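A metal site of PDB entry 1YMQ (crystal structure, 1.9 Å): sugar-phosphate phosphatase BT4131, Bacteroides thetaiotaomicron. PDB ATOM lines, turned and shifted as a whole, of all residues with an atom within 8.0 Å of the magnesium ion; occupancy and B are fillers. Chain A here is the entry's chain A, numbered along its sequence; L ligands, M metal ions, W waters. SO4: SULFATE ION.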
ATOM      1  N   PHE A   7     -11.863 -14.681   2.917  1.00  0.00           N
ATOM      2  CA  PHE A   7     -10.616 -15.275   3.399  1.00  0.00           C
ATOM      3  C   PHE A   7     -10.808 -16.372   4.417  1.00  0.00           C
ATOM      4  O   PHE A   7     -11.454 -16.173   5.453  1.00  0.00           O
ATOM      5  CB  PHE A   7      -9.734 -14.206   4.098  1.00  0.00           C
ATOM      6  CG  PHE A   7      -9.339 -13.081   3.231  1.00  0.00           C
ATOM      7  CD1 PHE A   7     -10.068 -11.901   3.208  1.00  0.00           C
ATOM      8  CD2 PHE A   7      -8.175 -13.183   2.423  1.00  0.00           C
ATOM      9  CE1 PHE A   7      -9.659 -10.808   2.382  1.00  0.00           C
ATOM     10  CE2 PHE A   7      -7.746 -12.143   1.611  1.00  0.00           C
ATOM     11  CZ  PHE A   7      -8.475 -10.956   1.569  1.00  0.00           C
ATOM     12  N   ASP A   8     -10.181 -17.488   4.148  1.00  0.00           N
ATOM     13  CA  ASP A   8     -10.109 -18.572   5.132  1.00  0.00           C
ATOM     14  C   ASP A   8      -9.127 -18.021   6.199  1.00  0.00           C
ATOM     15  O   ASP A   8      -8.316 -17.125   5.920  1.00  0.00           O
ATOM     16  CB  ASP A   8      -9.491 -19.798   4.461  1.00  0.00           C
ATOM     17  CG  ASP A   8      -9.100 -20.817   5.447  1.00  0.00           C
ATOM     18  OD1 ASP A   8      -7.969 -21.302   5.326  1.00  0.00           O
ATOM     19  OD2 ASP A   8      -9.954 -21.100   6.345  1.00  0.00           O
ATOM     20  N   ILE A   9      -9.168 -18.547   7.407  1.00  0.00           N
ATOM     21  CA  ILE A   9      -8.251 -18.018   8.436  1.00  0.00           C
ATOM     22  C   ILE A   9      -6.917 -18.766   8.478  1.00  0.00           C
ATOM     23  O   ILE A   9      -5.881 -18.239   8.043  1.00  0.00           O
ATOM     24  CB  ILE A   9      -8.875 -18.120   9.869  1.00  0.00           C
ATOM     25  CG1 ILE A   9     -10.111 -17.227   9.945  1.00  0.00           C
ATOM     26  CG2 ILE A   9      -7.827 -17.650  10.960  1.00  0.00           C
ATOM     27  CD1 ILE A   9     -10.934 -17.314  11.314  1.00  0.00           C
ATOM     28  N   ASP A  10      -6.956 -19.992   8.968  1.00  0.00           N
ATOM     29  CA  ASP A  10      -5.747 -20.782   9.188  1.00  0.00           C
ATOM     30  C   ASP A  10      -5.009 -21.230   7.933  1.00  0.00           C
ATOM     31  O   ASP A  10      -5.505 -22.037   7.172  1.00  0.00           O
ATOM     32  CB  ASP A  10      -6.080 -21.982  10.103  1.00  0.00           C
ATOM     33  CG  ASP A  10      -6.714 -21.545  11.394  1.00  0.00           C
ATOM     34  OD1 ASP A  10      -6.046 -20.865  12.205  1.00  0.00           O
ATOM     35  OD2 ASP A  10      -7.916 -21.846  11.601  1.00  0.00           O
ATOM     36  N   GLY A  11      -3.789 -20.712   7.764  1.00  0.00           N
ATOM     37  CA  GLY A  11      -3.022 -21.042   6.578  1.00  0.00           C
ATOM     38  C   GLY A  11      -3.295 -20.044   5.434  1.00  0.00           C
ATOM     39  O   GLY A  11      -2.659 -20.128   4.393  1.00  0.00           O
ATOM     40  N   THR A  12      -4.217 -19.090   5.617  1.00  0.00           N
ATOM     41  CA  THR A  12      -4.523 -18.119   4.549  1.00  0.00           C
ATOM     42  C   THR A  12      -4.258 -16.700   5.072  1.00  0.00           C
ATOM     43  O   THR A  12      -3.471 -15.964   4.500  1.00  0.00           O
ATOM     44  CB  THR A  12      -5.958 -18.350   4.070  1.00  0.00           C
ATOM     45  OG1 THR A  12      -6.042 -19.672   3.511  1.00  0.00           O
ATOM     46  CG2 THR A  12      -6.352 -17.307   3.007  1.00  0.00           C
ATOM     47  N   LEU A  13      -4.874 -16.344   6.200  1.00  0.00           N
ATOM     48  CA  LEU A  13      -4.590 -15.080   6.882  1.00  0.00           C
ATOM     49  C   LEU A  13      -3.507 -15.307   7.958  1.00  0.00           C
ATOM     50  O   LEU A  13      -2.539 -14.564   8.078  1.00  0.00           O
ATOM     51  CB  LEU A  13      -5.851 -14.558   7.596  1.00  0.00           C
ATOM     52  CG  LEU A  13      -6.953 -14.050   6.610  1.00  0.00           C
ATOM     53  CD1 LEU A  13      -8.262 -13.783   7.349  1.00  0.00           C
ATOM     54  CD2 LEU A  13      -6.435 -12.752   5.921  1.00  0.00           C
ATOM     55  N   VAL A  14      -3.708 -16.348   8.774  1.00  0.00           N
ATOM     56  CA  VAL A  14      -2.817 -16.619   9.925  1.00  0.00           C
ATOM     57  C   VAL A  14      -1.897 -17.772   9.616  1.00  0.00           C
ATOM     58  O   VAL A  14      -2.358 -18.806   9.180  1.00  0.00           O
ATOM     59  CB  VAL A  14      -3.636 -17.029  11.170  1.00  0.00           C
ATOM     60  CG1 VAL A  14      -2.736 -17.212  12.370  1.00  0.00           C
ATOM     61  CG2 VAL A  14      -4.691 -15.920  11.489  1.00  0.00           C
ATOM     62  N   PHE A  16       0.453 -20.936  10.170  1.00  0.00           N
ATOM     63  CA  PHE A  16       0.480 -22.080  11.083  1.00  0.00           C
ATOM     64  C   PHE A  16       1.886 -22.043  11.701  1.00  0.00           C
ATOM     65  O   PHE A  16       2.087 -22.466  12.821  1.00  0.00           O
ATOM     66  CB  PHE A  16       0.335 -23.402  10.327  1.00  0.00           C
ATOM     67  CG  PHE A  16      -1.089 -23.832  10.088  1.00  0.00           C
ATOM     68  CD1 PHE A  16      -1.908 -24.151  11.151  1.00  0.00           C
ATOM     69  CD2 PHE A  16      -1.593 -23.884   8.791  1.00  0.00           C
ATOM     70  CE1 PHE A  16      -3.248 -24.516  10.931  1.00  0.00           C
ATOM     71  CE2 PHE A  16      -2.898 -24.240   8.552  1.00  0.00           C
ATOM     72  CZ  PHE A  16      -3.747 -24.557   9.628  1.00  0.00           C
ATOM     73  N   ALA A  42     -14.159 -16.656   6.123  1.00  0.00           N
ATOM     74  CA  ALA A  42     -14.879 -17.872   5.719  1.00  0.00           C
ATOM     75  C   ALA A  42     -14.025 -18.980   6.319  1.00  0.00           C
ATOM     76  O   ALA A  42     -13.020 -19.406   5.737  1.00  0.00           O
ATOM     77  CB  ALA A  42     -14.992 -17.995   4.149  1.00  0.00           C
ATOM     78  N   THR A  43     -14.454 -19.425   7.489  1.00  0.00           N
ATOM     79  CA  THR A  43     -13.709 -20.397   8.283  1.00  0.00           C
ATOM     80  C   THR A  43     -14.520 -21.622   8.740  1.00  0.00           C
ATOM     81  O   THR A  43     -15.752 -21.580   8.816  1.00  0.00           O
ATOM     82  CB  THR A  43     -13.118 -19.678   9.539  1.00  0.00           C
ATOM     83  OG1 THR A  43     -12.266 -20.595  10.263  1.00  0.00           O
ATOM     84  CG2 THR A  43     -14.227 -19.114  10.452  1.00  0.00           C
ATOM     85  N   GLY A  44     -13.800 -22.740   8.962  1.00  0.00           N
ATOM     86  CA  GLY A  44     -14.447 -23.934   9.477  1.00  0.00           C
ATOM     87  C   GLY A  44     -14.545 -23.752  10.977  1.00  0.00           C
ATOM     88  O   GLY A  44     -15.243 -24.512  11.654  1.00  0.00           O
ATOM     89  N   TRP A 174      -8.981 -30.381   6.019  1.00  0.00           N
ATOM     90  CA  TRP A 174      -7.754 -29.752   5.592  1.00  0.00           C
ATOM     91  C   TRP A 174      -6.618 -30.392   6.397  1.00  0.00           C
ATOM     92  O   TRP A 174      -5.440 -30.195   6.106  1.00  0.00           O
ATOM     93  CB  TRP A 174      -7.832 -28.252   5.834  1.00  0.00           C
ATOM     94  CG  TRP A 174      -8.102 -27.882   7.241  1.00  0.00           C
ATOM     95  CD1 TRP A 174      -9.304 -27.609   7.800  1.00  0.00           C
ATOM     96  CD2 TRP A 174      -7.125 -27.718   8.256  1.00  0.00           C
ATOM     97  NE1 TRP A 174      -9.143 -27.261   9.126  1.00  0.00           N
ATOM     98  CE2 TRP A 174      -7.805 -27.329   9.439  1.00  0.00           C
ATOM     99  CE3 TRP A 174      -5.730 -27.843   8.297  1.00  0.00           C
ATOM    100  CZ2 TRP A 174      -7.141 -27.087  10.634  1.00  0.00           C
ATOM    101  CZ3 TRP A 174      -5.072 -27.609   9.490  1.00  0.00           C
ATOM    102  CH2 TRP A 174      -5.776 -27.232  10.637  1.00  0.00           C
ATOM    103  N   LYS A 188     -18.385 -23.469   2.518  1.00  0.00           N
ATOM    104  CA  LYS A 188     -18.098 -22.023   2.366  1.00  0.00           C
ATOM    105  C   LYS A 188     -18.749 -21.417   1.148  1.00  0.00           C
ATOM    106  O   LYS A 188     -19.034 -20.222   1.140  1.00  0.00           O
ATOM    107  CB  LYS A 188     -16.578 -21.808   2.386  1.00  0.00           C
ATOM    108  CG  LYS A 188     -16.000 -22.122   3.805  1.00  0.00           C
ATOM    109  CD  LYS A 188     -14.418 -22.062   3.784  1.00  0.00           C
ATOM    110  CE  LYS A 188     -13.856 -22.551   5.178  1.00  0.00           C
ATOM    111  NZ  LYS A 188     -12.402 -22.243   5.251  1.00  0.00           N
ATOM    112  N   PHE A 209     -10.013 -16.827  -1.054  1.00  0.00           N
ATOM    113  CA  PHE A 209      -8.623 -17.192  -0.807  1.00  0.00           C
ATOM    114  C   PHE A 209      -8.648 -18.351   0.176  1.00  0.00           C
ATOM    115  O   PHE A 209      -9.303 -18.276   1.205  1.00  0.00           O
ATOM    116  CB  PHE A 209      -7.821 -16.058  -0.169  1.00  0.00           C
ATOM    117  CG  PHE A 209      -7.838 -14.753  -0.926  1.00  0.00           C
ATOM    118  CD1 PHE A 209      -8.995 -13.959  -0.947  1.00  0.00           C
ATOM    119  CD2 PHE A 209      -6.699 -14.346  -1.633  1.00  0.00           C
ATOM    120  CE1 PHE A 209      -9.028 -12.761  -1.675  1.00  0.00           C
ATOM    121  CE2 PHE A 209      -6.715 -13.151  -2.384  1.00  0.00           C
ATOM    122  CZ  PHE A 209      -7.854 -12.369  -2.398  1.00  0.00           C
ATOM    123  N   GLY A 210      -7.886 -19.389  -0.134  1.00  0.00           N
ATOM    124  CA  GLY A 210      -7.856 -20.561   0.750  1.00  0.00           C
ATOM    125  C   GLY A 210      -6.646 -21.448   0.582  1.00  0.00           C
ATOM    126  O   GLY A 210      -5.950 -21.383  -0.434  1.00  0.00           O
ATOM    127  N   ASP A 211      -6.410 -22.330   1.574  1.00  0.00           N
ATOM    128  CA  ASP A 211      -5.269 -23.254   1.501  1.00  0.00           C
ATOM    129  C   ASP A 211      -5.664 -24.712   1.778  1.00  0.00           C
ATOM    130  O   ASP A 211      -4.830 -25.562   1.694  1.00  0.00           O
ATOM    131  CB  ASP A 211      -4.235 -22.922   2.601  1.00  0.00           C
ATOM    132  CG  ASP A 211      -4.727 -23.295   3.964  1.00  0.00           C
ATOM    133  OD1 ASP A 211      -5.872 -22.938   4.297  1.00  0.00           O
ATOM    134  OD2 ASP A 211      -3.969 -23.936   4.706  1.00  0.00           O
ATOM    135  N   GLY A 212      -6.942 -24.978   2.093  1.00  0.00           N
ATOM    136  CA  GLY A 212      -7.329 -26.312   2.494  1.00  0.00           C
ATOM    137  C   GLY A 212      -8.473 -26.966   1.756  1.00  0.00           C
ATOM    138  O   GLY A 212      -9.182 -26.333   0.989  1.00  0.00           O
ATOM    139  N   GLY A 213      -8.644 -28.272   2.013  1.00  0.00           N
ATOM    140  CA  GLY A 213      -9.686 -29.014   1.328  1.00  0.00           C
ATOM    141  C   GLY A 213     -11.088 -28.416   1.514  1.00  0.00           C
ATOM    142  O   GLY A 213     -11.866 -28.439   0.559  1.00  0.00           O
ATOM    143  N   ASN A 214     -11.397 -27.881   2.691  1.00  0.00           N
ATOM    144  CA  ASN A 214     -12.703 -27.299   2.942  1.00  0.00           C
ATOM    145  C   ASN A 214     -12.882 -25.927   2.232  1.00  0.00           C
ATOM    146  O   ASN A 214     -13.927 -25.307   2.373  1.00  0.00           O
ATOM    147  CB  ASN A 214     -13.027 -27.183   4.458  1.00  0.00           C
ATOM    148  CG  ASN A 214     -12.067 -26.271   5.210  1.00  0.00           C
ATOM    149  OD1 ASN A 214     -10.880 -26.176   4.885  1.00  0.00           O
ATOM    150  ND2 ASN A 214     -12.568 -25.623   6.261  1.00  0.00           N
ATOM    151  N   ASP A 215     -11.890 -25.526   1.432  1.00  0.00           N
ATOM    152  CA  ASP A 215     -11.944 -24.273   0.680  1.00  0.00           C
ATOM    153  C   ASP A 215     -12.206 -24.544  -0.787  1.00  0.00           C
ATOM    154  O   ASP A 215     -12.467 -23.625  -1.536  1.00  0.00           O
ATOM    155  CB  ASP A 215     -10.620 -23.456   0.783  1.00  0.00           C
ATOM    156  CG  ASP A 215     -10.310 -23.028   2.194  1.00  0.00           C
ATOM    157  OD1 ASP A 215     -11.286 -22.622   2.864  1.00  0.00           O
ATOM    158  OD2 ASP A 215      -9.119 -23.077   2.642  1.00  0.00           O
ATOM    159  N   MET A 218     -15.458 -22.984  -2.243  1.00  0.00           N
ATOM    160  CA  MET A 218     -15.536 -21.534  -2.458  1.00  0.00           C
ATOM    161  C   MET A 218     -14.490 -21.048  -3.442  1.00  0.00           C
ATOM    162  O   MET A 218     -14.642 -19.980  -4.030  1.00  0.00           O
ATOM    163  CB  MET A 218     -15.446 -20.752  -1.127  1.00  0.00           C
ATOM    164  CG  MET A 218     -14.088 -20.770  -0.432  1.00  0.00           C
ATOM    165  SD  MET A 218     -14.045 -19.441   0.845  1.00  0.00           S
ATOM    166  CE  MET A 218     -12.347 -19.548   1.346  1.00  0.00           C
ATOM    167  N   MET A 228      -3.388 -20.580  -1.764  1.00  0.00           N
ATOM    168  CA  MET A 228      -2.128 -20.230  -1.148  1.00  0.00           C
ATOM    169  C   MET A 228      -1.027 -21.128  -1.737  1.00  0.00           C
ATOM    170  O   MET A 228      -1.287 -22.293  -2.083  1.00  0.00           O
ATOM    171  CB  MET A 228      -2.214 -20.408   0.373  1.00  0.00           C
ATOM    172  CG  MET A 228      -3.330 -19.477   1.037  1.00  0.00           C
ATOM    173  SD  MET A 228      -3.223 -17.742   0.477  1.00  0.00           S
ATOM    174  CE  MET A 228      -1.657 -17.143   1.302  1.00  0.00           C
ATOM    175  N   GLN A 230       1.335 -22.811  -0.540  1.00  0.00           N
ATOM    176  CA  GLN A 230       1.690 -24.042   0.117  1.00  0.00           C
ATOM    177  C   GLN A 230       0.498 -25.033   0.217  1.00  0.00           C
ATOM    178  O   GLN A 230       0.549 -26.029   0.915  1.00  0.00           O
ATOM    179  CB  GLN A 230       2.251 -23.718   1.510  1.00  0.00           C
ATOM    180  CG  GLN A 230       1.195 -23.479   2.684  1.00  0.00           C
ATOM    181  CD  GLN A 230       0.440 -22.093   2.623  1.00  0.00           C
ATOM    182  OE1 GLN A 230       0.856 -21.154   1.895  1.00  0.00           O
ATOM    183  NE2 GLN A 230      -0.668 -21.994   3.376  1.00  0.00           N
HETATM  184  S   SO4 L   1      -9.934 -22.653   8.682  1.00  0.00           S
HETATM  185  O1  SO4 L   1     -10.026 -21.187   8.829  1.00  0.00           O
HETATM  186  O2  SO4 L   1      -8.622 -22.999   8.002  1.00  0.00           O
HETATM  187  O3  SO4 L   1      -9.967 -23.250  10.067  1.00  0.00           O
HETATM  188  O4  SO4 L   1     -11.044 -23.283   7.878  1.00  0.00           O
HETATM  189 MG    MG M   1      -7.214 -23.159   6.182  1.00  0.00          MG
HETATM  190  O   HOH W   1      -5.795 -25.018   6.453  1.00  0.00           O
HETATM  191  O   HOH W   2      -8.798 -24.435   5.066  1.00  0.00           O
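Three residues have an atom within 4 Å of the magnesium ion: Asp 8, Asp 10 and Asp 211.
Water W2 lies within hydrogen-bond range of the side-chain amide oxygen (OD1) of Asn 214 (2.7 Å) and the side-chain carboxylate (OD2) of Asp 215 (2.8 Å).
The backbone NH of Asp 211 is in hydrogen-bond range of the side-chain hydroxyl of Thr 12 (3.3 Å). OD2 of Asp 215 is in hydrogen-bond range of N of Asp 211 (3.0 Å). The backbone NH (N) of Asp 8 sits at hydrogen-bond distance from the backbone carbonyl oxygen (O) of Phe 209, 3.2 Å away. OG1 of Thr 12 lies close to OD1 of Asp 8 (3.1 Å). The side-chain carboxylate (OD2) of Asp 8 is in salt-bridge range of the side-chain amino group (NZ) of Lys 188.
The magnesium ion is bound by OD1 of Asp 8, O of Asp 10, O2 of the ligand, water W2, OD1 of Asp 211 and water W1.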
